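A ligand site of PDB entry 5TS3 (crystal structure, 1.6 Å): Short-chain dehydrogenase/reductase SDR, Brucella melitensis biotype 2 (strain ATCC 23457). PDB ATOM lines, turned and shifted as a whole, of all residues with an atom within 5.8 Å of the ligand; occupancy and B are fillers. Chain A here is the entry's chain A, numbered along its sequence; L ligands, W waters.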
ATOM      1  N   THR A  33      -6.921 -20.019   4.932  1.00  0.00           N
ATOM      2  CA  THR A  33      -5.967 -20.815   5.696  1.00  0.00           C
ATOM      3  C   THR A  33      -6.271 -22.305   5.560  1.00  0.00           C
ATOM      4  O   THR A  33      -7.415 -22.713   5.364  1.00  0.00           O
ATOM      5  CB  THR A  33      -5.928 -20.418   7.175  1.00  0.00           C
ATOM      6  OG1 THR A  33      -7.155 -20.769   7.814  1.00  0.00           O
ATOM      7  CG2 THR A  33      -5.677 -18.913   7.337  1.00  0.00           C
ATOM      8  N   GLY A  34      -5.206 -23.110   5.647  1.00  0.00           N
ATOM      9  CA  GLY A  34      -5.354 -24.546   5.409  1.00  0.00           C
ATOM     10  C   GLY A  34      -5.729 -24.862   3.985  1.00  0.00           C
ATOM     11  O   GLY A  34      -6.483 -25.815   3.747  1.00  0.00           O
ATOM     12  N   ALA A  35      -5.222 -24.094   3.018  1.00  0.00           N
ATOM     13  CA  ALA A  35      -5.732 -24.137   1.653  1.00  0.00           C
ATOM     14  C   ALA A  35      -5.083 -25.205   0.785  1.00  0.00           C
ATOM     15  O   ALA A  35      -5.447 -25.327  -0.392  1.00  0.00           O
ATOM     16  CB  ALA A  35      -5.558 -22.769   0.994  1.00  0.00           C
ATOM     17  N   ALA A  36      -4.132 -26.001   1.301  1.00  0.00           N
ATOM     18  CA  ALA A  36      -3.397 -26.922   0.433  1.00  0.00           C
ATOM     19  C   ALA A  36      -3.971 -28.339   0.401  1.00  0.00           C
ATOM     20  O   ALA A  36      -3.471 -29.165  -0.365  1.00  0.00           O
ATOM     21  CB  ALA A  36      -1.924 -26.996   0.840  1.00  0.00           C
ATOM     22  N   ARG A  37      -5.003 -28.614   1.185  1.00  0.00           N
ATOM     23  CA  ARG A  37      -5.608 -29.937   1.219  1.00  0.00           C
ATOM     24  C   ARG A  37      -7.046 -29.790   1.687  1.00  0.00           C
ATOM     25  O   ARG A  37      -7.413 -28.785   2.302  1.00  0.00           O
ATOM     26  CB  ARG A  37      -4.842 -30.884   2.163  1.00  0.00           C
ATOM     27  CG  ARG A  37      -5.286 -32.336   2.110  1.00  0.00           C
ATOM     28  CD  ARG A  37      -4.455 -33.214   3.046  1.00  0.00           C
ATOM     29  NE  ARG A  37      -4.620 -32.850   4.450  1.00  0.00           N
ATOM     30  CZ  ARG A  37      -3.829 -33.296   5.420  1.00  0.00           C
ATOM     31  NH1 ARG A  37      -2.828 -34.127   5.132  1.00  0.00           N
ATOM     32  NH2 ARG A  37      -4.032 -32.919   6.688  1.00  0.00           N
ATOM     33  N   GLY A  38      -7.869 -30.795   1.377  1.00  0.00           N
ATOM     34  CA  GLY A  38      -9.168 -30.906   2.026  1.00  0.00           C
ATOM     35  C   GLY A  38     -10.147 -29.789   1.666  1.00  0.00           C
ATOM     36  O   GLY A  38     -10.174 -29.289   0.531  1.00  0.00           O
ATOM     37  N   ILE A  39     -10.955 -29.399   2.650  1.00  0.00           N
ATOM     38  CA  ILE A  39     -11.970 -28.386   2.407  1.00  0.00           C
ATOM     39  C   ILE A  39     -11.337 -27.065   1.995  1.00  0.00           C
ATOM     40  O   ILE A  39     -11.830 -26.373   1.096  1.00  0.00           O
ATOM     41  CB  ILE A  39     -12.877 -28.232   3.648  1.00  0.00           C
ATOM     42  CG1 ILE A  39     -13.638 -29.534   3.944  1.00  0.00           C
ATOM     43  CG2 ILE A  39     -13.850 -27.065   3.464  1.00  0.00           C
ATOM     44  CD1 ILE A  39     -14.415 -29.513   5.288  1.00  0.00           C
ATOM     45  N   GLY A  40     -10.214 -26.694   2.624  1.00  0.00           N
ATOM     46  CA  GLY A  40      -9.552 -25.447   2.262  1.00  0.00           C
ATOM     47  C   GLY A  40      -9.124 -25.405   0.813  1.00  0.00           C
ATOM     48  O   GLY A  40      -9.214 -24.369   0.152  1.00  0.00           O
ATOM     49  N   CYS A  57      -2.690 -20.122   2.186  1.00  0.00           N
ATOM     50  CA  CYS A  57      -1.974 -20.220   3.456  1.00  0.00           C
ATOM     51  C   CYS A  57      -1.975 -21.669   3.936  1.00  0.00           C
ATOM     52  O   CYS A  57      -3.050 -22.251   4.135  1.00  0.00           O
ATOM     53  CB  CYS A  57      -2.576 -19.287   4.498  1.00  0.00           C
ATOM     54  SG  CYS A  57      -1.913 -19.512   6.167  1.00  0.00           S
ATOM     55  N   ASP A  58      -0.788 -22.251   4.075  1.00  0.00           N
ATOM     56  CA  ASP A  58      -0.647 -23.600   4.615  1.00  0.00           C
ATOM     57  C   ASP A  58       0.804 -23.743   5.077  1.00  0.00           C
ATOM     58  O   ASP A  58       1.618 -22.829   4.913  1.00  0.00           O
ATOM     59  CB  ASP A  58      -1.060 -24.663   3.586  1.00  0.00           C
ATOM     60  CG  ASP A  58      -1.667 -25.901   4.225  1.00  0.00           C
ATOM     61  OD1 ASP A  58      -0.940 -26.600   4.979  1.00  0.00           O
ATOM     62  OD2 ASP A  58      -2.877 -26.159   3.990  1.00  0.00           O
ATOM     63  N   LEU A  59       1.118 -24.902   5.660  1.00  0.00           N
ATOM     64  CA  LEU A  59       2.365 -25.061   6.421  1.00  0.00           C
ATOM     65  C   LEU A  59       3.589 -25.242   5.526  1.00  0.00           C
ATOM     66  O   LEU A  59       4.622 -24.618   5.752  1.00  0.00           O
ATOM     67  CB  LEU A  59       2.236 -26.244   7.382  1.00  0.00           C
ATOM     68  CG  LEU A  59       1.327 -26.048   8.590  1.00  0.00           C
ATOM     69  CD1 LEU A  59       0.943 -27.385   9.218  1.00  0.00           C
ATOM     70  CD2 LEU A  59       2.003 -25.160   9.628  1.00  0.00           C
ATOM     71  N   CYS A  84       3.036 -20.529   6.067  1.00  0.00           N
ATOM     72  CA  CYS A  84       3.292 -20.204   7.467  1.00  0.00           C
ATOM     73  C   CYS A  84       2.383 -21.051   8.344  1.00  0.00           C
ATOM     74  O   CYS A  84       1.439 -21.695   7.877  1.00  0.00           O
ATOM     75  CB  CYS A  84       3.090 -18.717   7.761  1.00  0.00           C
ATOM     76  SG  CYS A  84       1.391 -18.182   7.503  1.00  0.00           S
ATOM     77  N   ASP A  85       2.704 -21.041   9.635  1.00  0.00           N
ATOM     78  CA  ASP A  85       1.880 -21.624  10.681  1.00  0.00           C
ATOM     79  C   ASP A  85       0.968 -20.530  11.211  1.00  0.00           C
ATOM     80  O   ASP A  85       1.457 -19.544  11.781  1.00  0.00           O
ATOM     81  CB  ASP A  85       2.795 -22.168  11.791  1.00  0.00           C
ATOM     82  CG  ASP A  85       2.040 -22.871  12.904  1.00  0.00           C
ATOM     83  OD1 ASP A  85       0.848 -22.580  13.125  1.00  0.00           O
ATOM     84  OD2 ASP A  85       2.664 -23.714  13.573  1.00  0.00           O
ATOM     85  N   VAL A  86      -0.348 -20.685  11.024  1.00  0.00           N
ATOM     86  CA  VAL A  86      -1.290 -19.627  11.408  1.00  0.00           C
ATOM     87  C   VAL A  86      -1.244 -19.323  12.889  1.00  0.00           C
ATOM     88  O   VAL A  86      -1.661 -18.227  13.300  1.00  0.00           O
ATOM     89  CB  VAL A  86      -2.742 -19.966  11.010  1.00  0.00           C
ATOM     90  CG1 VAL A  86      -2.906 -20.015   9.505  1.00  0.00           C
ATOM     91  CG2 VAL A  86      -3.210 -21.264  11.676  1.00  0.00           C
ATOM     92  N   SER A  87      -0.757 -20.248  13.729  1.00  0.00           N
ATOM     93  CA  SER A  87      -0.661 -19.977  15.159  1.00  0.00           C
ATOM     94  C   SER A  87       0.496 -19.061  15.525  1.00  0.00           C
ATOM     95  O   SER A  87       0.550 -18.596  16.680  1.00  0.00           O
ATOM     96  CB  SER A  87      -0.539 -21.292  15.951  1.00  0.00           C
ATOM     97  OG  SER A  87       0.711 -21.955  15.721  1.00  0.00           O
ATOM     98  N   ASN A 108     -11.056 -18.609   7.551  1.00  0.00           N
ATOM     99  CA  ASN A 108     -10.293 -19.387   8.520  1.00  0.00           C
ATOM    100  C   ASN A 108     -10.742 -20.831   8.457  1.00  0.00           C
ATOM    101  O   ASN A 108     -11.757 -21.205   9.058  1.00  0.00           O
ATOM    102  CB  ASN A 108     -10.493 -18.828   9.919  1.00  0.00           C
ATOM    103  CG  ASN A 108      -9.708 -17.568  10.142  1.00  0.00           C
ATOM    104  OD1 ASN A 108      -8.470 -17.589  10.055  1.00  0.00           O
ATOM    105  ND2 ASN A 108     -10.403 -16.476  10.433  1.00  0.00           N
ATOM    106  N   ASN A 109      -9.984 -21.652   7.737  1.00  0.00           N
ATOM    107  CA  ASN A 109     -10.300 -23.066   7.585  1.00  0.00           C
ATOM    108  C   ASN A 109      -9.281 -23.987   8.228  1.00  0.00           C
ATOM    109  O   ASN A 109      -9.629 -25.110   8.586  1.00  0.00           O
ATOM    110  CB  ASN A 109     -10.472 -23.369   6.087  1.00  0.00           C
ATOM    111  CG  ASN A 109     -10.309 -24.836   5.761  1.00  0.00           C
ATOM    112  OD1 ASN A 109     -11.277 -25.594   5.741  1.00  0.00           O
ATOM    113  ND2 ASN A 109      -9.066 -25.244   5.480  1.00  0.00           N
ATOM    114  N   ALA A 110      -8.044 -23.526   8.427  1.00  0.00           N
ATOM    115  CA  ALA A 110      -7.046 -24.397   9.068  1.00  0.00           C
ATOM    116  C   ALA A 110      -7.545 -24.923  10.406  1.00  0.00           C
ATOM    117  O   ALA A 110      -8.089 -24.190  11.229  1.00  0.00           O
ATOM    118  CB  ALA A 110      -5.738 -23.644   9.266  1.00  0.00           C
ATOM    119  N   GLY A 111      -7.333 -26.220  10.627  1.00  0.00           N
ATOM    120  CA  GLY A 111      -7.774 -26.851  11.848  1.00  0.00           C
ATOM    121  C   GLY A 111      -7.160 -28.228  11.951  1.00  0.00           C
ATOM    122  O   GLY A 111      -6.805 -28.839  10.933  1.00  0.00           O
ATOM    123  N   ILE A 112      -7.010 -28.721  13.176  1.00  0.00           N
ATOM    124  CA  ILE A 112      -6.471 -30.055  13.412  1.00  0.00           C
ATOM    125  C   ILE A 112      -7.393 -30.792  14.382  1.00  0.00           C
ATOM    126  O   ILE A 112      -8.105 -30.189  15.186  1.00  0.00           O
ATOM    127  CB  ILE A 112      -5.024 -30.019  13.952  1.00  0.00           C
ATOM    128  CG1 ILE A 112      -4.912 -29.155  15.208  1.00  0.00           C
ATOM    129  CG2 ILE A 112      -4.037 -29.538  12.865  1.00  0.00           C
ATOM    130  CD1 ILE A 112      -3.551 -29.294  15.917  1.00  0.00           C
ATOM    131  N   ARG A 133      -1.898 -27.374  21.792  1.00  0.00           N
ATOM    132  CA  ARG A 133      -1.630 -27.211  20.368  1.00  0.00           C
ATOM    133  C   ARG A 133      -2.923 -27.069  19.577  1.00  0.00           C
ATOM    134  O   ARG A 133      -3.024 -26.216  18.681  1.00  0.00           O
ATOM    135  CB  ARG A 133      -0.799 -28.390  19.851  1.00  0.00           C
ATOM    136  CG  ARG A 133      -0.501 -28.321  18.360  1.00  0.00           C
ATOM    137  CD  ARG A 133       0.310 -27.079  18.006  1.00  0.00           C
ATOM    138  NE  ARG A 133       0.552 -26.985  16.564  1.00  0.00           N
ATOM    139  CZ  ARG A 133       1.005 -25.895  15.956  1.00  0.00           C
ATOM    140  NH1 ARG A 133       1.250 -24.794  16.641  1.00  0.00           N
ATOM    141  NH2 ARG A 133       1.194 -25.908  14.639  1.00  0.00           N
ATOM    142  N   VAL A 137      -3.917 -23.754  17.305  1.00  0.00           N
ATOM    143  CA  VAL A 137      -4.204 -23.763  15.874  1.00  0.00           C
ATOM    144  C   VAL A 137      -5.650 -23.411  15.590  1.00  0.00           C
ATOM    145  O   VAL A 137      -5.948 -22.537  14.775  1.00  0.00           O
ATOM    146  CB  VAL A 137      -3.845 -25.136  15.253  1.00  0.00           C
ATOM    147  CG1 VAL A 137      -4.286 -25.173  13.796  1.00  0.00           C
ATOM    148  CG2 VAL A 137      -2.354 -25.385  15.358  1.00  0.00           C
ATOM    149  N   ASN A 138      -6.585 -24.124  16.234  1.00  0.00           N
ATOM    150  CA  ASN A 138      -7.979 -24.042  15.828  1.00  0.00           C
ATOM    151  C   ASN A 138      -8.621 -22.733  16.264  1.00  0.00           C
ATOM    152  O   ASN A 138      -9.492 -22.188  15.572  1.00  0.00           O
ATOM    153  CB  ASN A 138      -8.787 -25.198  16.427  1.00  0.00           C
ATOM    154  CG  ASN A 138      -8.481 -26.522  15.779  1.00  0.00           C
ATOM    155  OD1 ASN A 138      -7.536 -26.655  15.001  1.00  0.00           O
ATOM    156  ND2 ASN A 138      -9.288 -27.527  16.100  1.00  0.00           N
ATOM    157  N   THR A 164     -14.487 -21.339  10.655  1.00  0.00           N
ATOM    158  CA  THR A 164     -14.927 -22.724  10.523  1.00  0.00           C
ATOM    159  C   THR A 164     -15.113 -23.333  11.916  1.00  0.00           C
ATOM    160  O   THR A 164     -14.134 -23.538  12.653  1.00  0.00           O
ATOM    161  CB  THR A 164     -13.966 -23.557   9.673  1.00  0.00           C
ATOM    162  OG1 THR A 164     -13.789 -22.921   8.398  1.00  0.00           O
ATOM    163  CG2 THR A 164     -14.547 -24.950   9.418  1.00  0.00           C
ATOM    164  N   SER A 165     -16.371 -23.610  12.258  1.00  0.00           N
ATOM    165  CA  SER A 165     -16.723 -24.364  13.454  1.00  0.00           C
ATOM    166  C   SER A 165     -16.886 -25.833  13.064  1.00  0.00           C
ATOM    167  O   SER A 165     -16.153 -26.339  12.211  1.00  0.00           O
ATOM    168  CB  SER A 165     -17.990 -23.761  14.082  1.00  0.00           C
ATOM    169  OG  SER A 165     -18.379 -24.409  15.285  1.00  0.00           O
ATOM    170  N   SER A 166     -17.839 -26.520  13.679  1.00  0.00           N
ATOM    171  CA  SER A 166     -18.163 -27.917  13.375  1.00  0.00           C
ATOM    172  C   SER A 166     -19.454 -28.227  14.117  1.00  0.00           C
ATOM    173  O   SER A 166     -19.726 -27.631  15.154  1.00  0.00           O
ATOM    174  CB  SER A 166     -17.062 -28.885  13.834  1.00  0.00           C
ATOM    175  OG  SER A 166     -17.544 -30.233  13.797  1.00  0.00           O
ATOM    176  N   VAL A 167     -20.226 -29.179  13.589  1.00  0.00           N
ATOM    177  CA  VAL A 167     -21.393 -29.623  14.371  1.00  0.00           C
ATOM    178  C   VAL A 167     -20.946 -30.151  15.732  1.00  0.00           C
ATOM    179  O   VAL A 167     -21.697 -30.076  16.709  1.00  0.00           O
ATOM    180  CB  VAL A 167     -22.226 -30.664  13.600  1.00  0.00           C
ATOM    181  CG1 VAL A 167     -22.849 -30.038  12.339  1.00  0.00           C
ATOM    182  CG2 VAL A 167     -21.417 -31.907  13.252  1.00  0.00           C
ATOM    183  N   TYR A 180     -10.955 -30.477  20.258  1.00  0.00           N
ATOM    184  CA  TYR A 180     -11.655 -30.121  19.034  1.00  0.00           C
ATOM    185  C   TYR A 180     -13.036 -29.540  19.333  1.00  0.00           C
ATOM    186  O   TYR A 180     -13.394 -28.490  18.814  1.00  0.00           O
ATOM    187  CB  TYR A 180     -11.781 -31.358  18.151  1.00  0.00           C
ATOM    188  CG  TYR A 180     -12.288 -31.049  16.757  1.00  0.00           C
ATOM    189  CD1 TYR A 180     -11.420 -30.611  15.759  1.00  0.00           C
ATOM    190  CD2 TYR A 180     -13.645 -31.180  16.446  1.00  0.00           C
ATOM    191  CE1 TYR A 180     -11.879 -30.333  14.489  1.00  0.00           C
ATOM    192  CE2 TYR A 180     -14.105 -30.904  15.186  1.00  0.00           C
ATOM    193  CZ  TYR A 180     -13.224 -30.482  14.196  1.00  0.00           C
ATOM    194  OH  TYR A 180     -13.693 -30.202  12.946  1.00  0.00           O
ATOM    195  N   LYS A 184     -14.087 -25.638  18.515  1.00  0.00           N
ATOM    196  CA  LYS A 184     -15.117 -25.352  17.521  1.00  0.00           C
ATOM    197  C   LYS A 184     -16.309 -24.659  18.177  1.00  0.00           C
ATOM    198  O   LYS A 184     -16.961 -23.806  17.558  1.00  0.00           O
ATOM    199  CB  LYS A 184     -15.522 -26.646  16.805  1.00  0.00           C
ATOM    200  CG  LYS A 184     -14.400 -27.266  15.928  1.00  0.00           C
ATOM    201  CD  LYS A 184     -13.726 -26.200  15.045  1.00  0.00           C
ATOM    202  CE  LYS A 184     -12.849 -26.829  13.969  1.00  0.00           C
ATOM    203  NZ  LYS A 184     -12.369 -25.800  12.992  1.00  0.00           N
ATOM    204  N   ALA A 209     -20.356 -24.587  10.030  1.00  0.00           N
ATOM    205  CA  ALA A 209     -20.186 -25.756  10.890  1.00  0.00           C
ATOM    206  C   ALA A 209     -20.433 -27.007  10.059  1.00  0.00           C
ATOM    207  O   ALA A 209     -21.544 -27.553  10.045  1.00  0.00           O
ATOM    208  CB  ALA A 209     -21.117 -25.712  12.104  1.00  0.00           C
ATOM    209  N   PRO A 210     -19.413 -27.501   9.360  1.00  0.00           N
ATOM    210  CA  PRO A 210     -19.605 -28.710   8.546  1.00  0.00           C
ATOM    211  C   PRO A 210     -19.906 -29.921   9.407  1.00  0.00           C
ATOM    212  O   PRO A 210     -19.535 -29.994  10.584  1.00  0.00           O
ATOM    213  CB  PRO A 210     -18.265 -28.853   7.798  1.00  0.00           C
ATOM    214  CG  PRO A 210     -17.685 -27.456   7.786  1.00  0.00           C
ATOM    215  CD  PRO A 210     -18.079 -26.908   9.147  1.00  0.00           C
ATOM    216  N   GLY A 211     -20.598 -30.886   8.814  1.00  0.00           N
ATOM    217  CA  GLY A 211     -20.888 -32.143   9.481  1.00  0.00           C
ATOM    218  C   GLY A 211     -19.829 -33.188   9.187  1.00  0.00           C
ATOM    219  O   GLY A 211     -18.790 -33.223   9.843  1.00  0.00           O
ATOM    220  N   ARG A 212     -20.111 -34.077   8.242  1.00  0.00           N
ATOM    221  CA  ARG A 212     -19.145 -35.076   7.781  1.00  0.00           C
ATOM    222  C   ARG A 212     -18.947 -34.867   6.295  1.00  0.00           C
ATOM    223  O   ARG A 212     -19.869 -35.104   5.505  1.00  0.00           O
ATOM    224  CB  ARG A 212     -19.620 -36.501   8.079  1.00  0.00           C
ATOM    225  CG  ARG A 212     -19.636 -36.879   9.533  1.00  0.00           C
ATOM    226  CD  ARG A 212     -18.240 -36.917  10.143  1.00  0.00           C
ATOM    227  NE  ARG A 212     -17.260 -37.539   9.258  1.00  0.00           N
ATOM    228  CZ  ARG A 212     -17.118 -38.853   9.095  1.00  0.00           C
ATOM    229  NH1 ARG A 212     -16.188 -39.329   8.264  1.00  0.00           N
ATOM    230  NH2 ARG A 212     -17.917 -39.699   9.738  1.00  0.00           N
ATOM    231  N   ILE A 213     -17.748 -34.446   5.914  1.00  0.00           N
ATOM    232  CA  ILE A 213     -17.408 -34.082   4.542  1.00  0.00           C
ATOM    233  C   ILE A 213     -16.457 -35.118   3.978  1.00  0.00           C
ATOM    234  O   ILE A 213     -15.559 -35.592   4.678  1.00  0.00           O
ATOM    235  CB  ILE A 213     -16.774 -32.670   4.499  1.00  0.00           C
ATOM    236  CG1 ILE A 213     -17.654 -31.691   5.277  1.00  0.00           C
ATOM    237  CG2 ILE A 213     -16.610 -32.196   3.054  1.00  0.00           C
ATOM    238  CD1 ILE A 213     -19.103 -31.570   4.749  1.00  0.00           C
ATOM    239  N   ALA A 214     -16.660 -35.470   2.713  1.00  0.00           N
ATOM    240  CA  ALA A 214     -15.796 -36.413   2.002  1.00  0.00           C
ATOM    241  C   ALA A 214     -14.413 -35.790   1.853  1.00  0.00           C
ATOM    242  O   ALA A 214     -14.173 -34.972   0.964  1.00  0.00           O
ATOM    243  CB  ALA A 214     -16.399 -36.755   0.635  1.00  0.00           C
ATOM    244  N   THR A 215     -13.520 -36.153   2.751  1.00  0.00           N
ATOM    245  CA  THR A 215     -12.190 -35.563   2.897  1.00  0.00           C
ATOM    246  C   THR A 215     -11.222 -36.677   3.277  1.00  0.00           C
ATOM    247  O   THR A 215     -11.655 -37.798   3.582  1.00  0.00           O
ATOM    248  CB  THR A 215     -12.197 -34.492   3.975  1.00  0.00           C
ATOM    249  OG1 THR A 215     -12.862 -35.032   5.113  1.00  0.00           O
ATOM    250  CG2 THR A 215     -12.910 -33.221   3.497  1.00  0.00           C
ATOM    251  N   PRO A 216      -9.906 -36.435   3.255  1.00  0.00           N
ATOM    252  CA  PRO A 216      -8.959 -37.474   3.689  1.00  0.00           C
ATOM    253  C   PRO A 216      -9.244 -38.014   5.084  1.00  0.00           C
ATOM    254  O   PRO A 216      -8.972 -39.192   5.337  1.00  0.00           O
ATOM    255  CB  PRO A 216      -7.602 -36.740   3.632  1.00  0.00           C
ATOM    256  CG  PRO A 216      -7.776 -35.721   2.585  1.00  0.00           C
ATOM    257  CD  PRO A 216      -9.203 -35.262   2.697  1.00  0.00           C
ATOM    258  N   MET A 217      -9.798 -37.209   5.982  1.00  0.00           N
ATOM    259  CA  MET A 217     -10.119 -37.682   7.324  1.00  0.00           C
ATOM    260  C   MET A 217     -11.039 -38.910   7.315  1.00  0.00           C
ATOM    261  O   MET A 217     -11.057 -39.662   8.300  1.00  0.00           O
ATOM    262  CB  MET A 217     -10.776 -36.560   8.141  1.00  0.00           C
HETATM  263  P1  LIG L   1      -7.369 -31.460   6.467  1.00  0.00           P
HETATM  264  O1  LIG L   1      -6.528 -32.050   7.547  1.00  0.00           O
HETATM  265  O2  LIG L   1      -7.603 -32.354   5.270  1.00  0.00           O
HETATM  266  O3  LIG L   1      -6.767 -30.075   5.919  1.00  0.00           O
HETATM  267  C1  LIG L   1      -6.419 -29.044   6.851  1.00  0.00           C
HETATM  268  C2  LIG L   1      -5.329 -28.228   6.219  1.00  0.00           C
HETATM  269  O4  LIG L   1      -4.905 -27.220   7.166  1.00  0.00           O
HETATM  270  C3  LIG L   1      -4.071 -29.015   5.820  1.00  0.00           C
HETATM  271  O5  LIG L   1      -3.613 -28.650   4.525  1.00  0.00           O
HETATM  272  C4  LIG L   1      -3.077 -28.639   6.927  1.00  0.00           C
HETATM  273  O6  LIG L   1      -1.710 -28.678   6.523  1.00  0.00           O
HETATM  274  C5  LIG L   1      -3.490 -27.198   7.204  1.00  0.00           C
HETATM  275  N1  LIG L   1      -3.080 -26.721   8.523  1.00  0.00           N
HETATM  276  C6  LIG L   1      -3.109 -27.412   9.703  1.00  0.00           C
HETATM  277  N2  LIG L   1      -2.572 -26.768  10.713  1.00  0.00           N
HETATM  278  C7  LIG L   1      -2.162 -25.566  10.153  1.00  0.00           C
HETATM  279  C8  LIG L   1      -1.498 -24.453  10.691  1.00  0.00           C
HETATM  280  N3  LIG L   1      -1.119 -24.367  11.975  1.00  0.00           N
HETATM  281  N4  LIG L   1      -1.224 -23.418   9.872  1.00  0.00           N
HETATM  282  C9  LIG L   1      -1.603 -23.504   8.588  1.00  0.00           C
HETATM  283  N5  LIG L   1      -2.234 -24.504   7.965  1.00  0.00           N
HETATM  284  C10 LIG L   1      -2.483 -25.516   8.813  1.00  0.00           C
HETATM  285  O7  LIG L   1      -8.766 -31.022   7.104  1.00  0.00           O
HETATM  286  P2  LIG L   1     -10.236 -30.750   6.574  1.00  0.00           P
HETATM  287  O8  LIG L   1     -11.023 -31.976   6.852  1.00  0.00           O
HETATM  288  O9  LIG L   1     -10.203 -30.185   5.202  1.00  0.00           O
HETATM  289  O10 LIG L   1     -10.679 -29.623   7.606  1.00  0.00           O
HETATM  290  C11 LIG L   1     -10.789 -28.252   7.208  1.00  0.00           C
HETATM  291  C12 LIG L   1     -11.554 -27.521   8.300  1.00  0.00           C
HETATM  292  O11 LIG L   1     -12.915 -27.999   8.338  1.00  0.00           O
HETATM  293  C13 LIG L   1     -10.993 -27.704   9.717  1.00  0.00           C
HETATM  294  O12 LIG L   1     -11.147 -26.502  10.452  1.00  0.00           O
HETATM  295  C14 LIG L   1     -11.897 -28.798  10.284  1.00  0.00           C
HETATM  296  O13 LIG L   1     -11.986 -28.746  11.705  1.00  0.00           O
HETATM  297  C15 LIG L   1     -13.224 -28.399   9.645  1.00  0.00           C
HETATM  298  N6  LIG L   1     -14.251 -29.518   9.584  1.00  0.00           N
HETATM  299  C16 LIG L   1     -14.032 -30.575   8.784  1.00  0.00           C
HETATM  300  C17 LIG L   1     -14.965 -31.597   8.714  1.00  0.00           C
HETATM  301  C18 LIG L   1     -14.803 -32.794   7.816  1.00  0.00           C
HETATM  302  O14 LIG L   1     -15.690 -33.654   7.775  1.00  0.00           O
HETATM  303  N7  LIG L   1     -13.700 -32.881   7.079  1.00  0.00           N
HETATM  304  C19 LIG L   1     -16.123 -31.498   9.487  1.00  0.00           C
HETATM  305  C20 LIG L   1     -16.316 -30.399  10.300  1.00  0.00           C
HETATM  306  C21 LIG L   1     -15.364 -29.413  10.334  1.00  0.00           C
HETATM  307  O   HOH W   1      -8.664 -27.988   4.692  1.00  0.00           O
HETATM  308  O   HOH W   2     -15.751 -34.952  10.319  1.00  0.00           O
HETATM  309  O   HOH W   3     -15.136 -32.741  12.573  1.00  0.00           O
HETATM  310  O   HOH W   4      -5.767 -31.173   9.985  1.00  0.00           O
HETATM  311  O   HOH W   5       0.006 -30.710   7.388  1.00  0.00           O
HETATM  312  O   HOH W   6      -9.534 -34.251   5.781  1.00  0.00           O
HETATM  313  O   HOH W   7      -1.563 -30.032   3.149  1.00  0.00           O
HETATM  314  O   HOH W   8     -10.587 -23.338  11.085  1.00  0.00           O
HETATM  315  O   HOH W   9      -0.890 -27.599  12.865  1.00  0.00           O
HETATM  316  O   HOH W  10      -3.022 -30.891   9.564  1.00  0.00           O
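An oxygen (O13) of the ligand lies within hydrogen-bond range of the side-chain hydroxyl of Tyr 180.
OD2 of Asp 58 lies within hydrogen-bond range of O5 of the ligand.
N of Ile 39 lies within hydrogen-bond range of O9 of the ligand.
The guanidinium group of Arg 37 lies within salt-bridge range of an oxygen (O1) of the ligand (2.8 Å).
The backbone carbonyl oxygen (O) of Asn 109 lies within hydrogen-bond range of an oxygen (O12) of the ligand (2.8 Å).
The backbone NH of Ile 213 is in hydrogen-bond range of an oxygen (O14) of the ligand, 2.9 Å away.
N3 of the ligand lies within hydrogen-bond range of OD1 of Asp 85 (2.9 Å).
An oxygen (O12) of the ligand lies within hydrogen-bond range of the side-chain amino group (NZ) of Lys 184 (2.9 Å).
The side-chain hydroxyl of Thr 215 lies within hydrogen-bond range of a nitrogen (N7) of the ligand, at 3.0 Å.
The backbone NH of Val 86 is in hydrogen-bond range of a nitrogen (N4) of the ligand.
The side-chain carboxylate (OD2) of Asp 58 is in hydrogen-bond range of the backbone NH (N) of Ala 36, at 3.0 Å.
OD2 of Asp 58 lies within hydrogen-bond range of N of Ala 35 (3.3 Å).
N of Asn 109 is in hydrogen-bond range of OG1 of Thr 33 (3.0 Å).
The side-chain carboxylate (OD1) of Asp 85 lies within hydrogen-bond range of the side-chain hydroxyl (OG) of Ser 87 (2.7 Å).
O of Lys 184 sits at hydrogen-bond distance from OG of Ser 165 (2.7 Å).
The backbone NH (N) of Val 167 sits at hydrogen-bond distance from the backbone carbonyl oxygen (O) of Pro 210 (3.2 Å).
OG1 of Thr 164 lies within hydrogen-bond range of O of Asn 108, at 2.7 Å.
The backbone NH (N) of Ala 110 is in hydrogen-bond range of the side-chain hydroxyl (OG1) of Thr 33, 3.0 Å away.
Gly 34 touches the ligand (CA to O4, 3.2 Å).
Gly 38 touches the ligand (CA to O9, 3.4 Å).
CD2 of Leu 59 touches N4 of the ligand, 3.7 Å away.
O of Cys 84 touches C9 of the ligand (3.6 Å).
CB of Ala 110 touches C10 of the ligand, 3.8 Å away.
Gly 111 touches the ligand.
Ile 112 touches the ligand (CG2 to N2, 3.8 Å).
Arg 133 touches the ligand.
Val 137 touches the ligand.
Thr 164 touches the ligand (CG2 to O11, 3.6 Å).
O of Ser 165 touches C21 of the ligand, 3.7 Å away.
Ser 166 touches the ligand.
O of Pro 210 touches C20 of the ligand, 3.3 Å away.
Gly 211 touches the ligand.
Arg 212 touches the ligand.
Hydrophobic or aromatic side chains that line the ligand: Ile 39, Leu 59, Val 86, Ala 110, Ile 112, Val 137, Tyr 180, Pro 210 and Ile 213.
25 residues have an atom within 4 Å of the ligand: Gly 34, Arg 37, Gly 38, Ile 39, Asp 58, Leu 59, Cys 84, Asp 85, Val 86, Asn 109, Ala 110, Gly 111, Ile 112, Arg 133, Val 137, Thr 164, Ser 165, Ser 166, Tyr 180, Lys 184, Pro 210, Gly 211, Arg 212, Ile 213 and Thr 215.
The nearest printed residue that does not touch the ligand is Ala 36 (4.2 Å).
Water W4 bridges an oxygen (O1) of the ligand (2.7 Å) and the backbone carbonyl oxygen of Gly 111 (2.7 Å).
Water W6 lies within hydrogen-bond range of O2 of the ligand (2.8 Å), N of Met 217 (3.0 Å) and OG1 of Thr 215 (3.5 Å).
Water W9 bridges N2 of the ligand (2.9 Å) and NH2 of Arg 133 (3.2 Å).
Water W2 bridges O14 of the ligand (2.9 Å) and NE of Arg 212 (3.2 Å).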
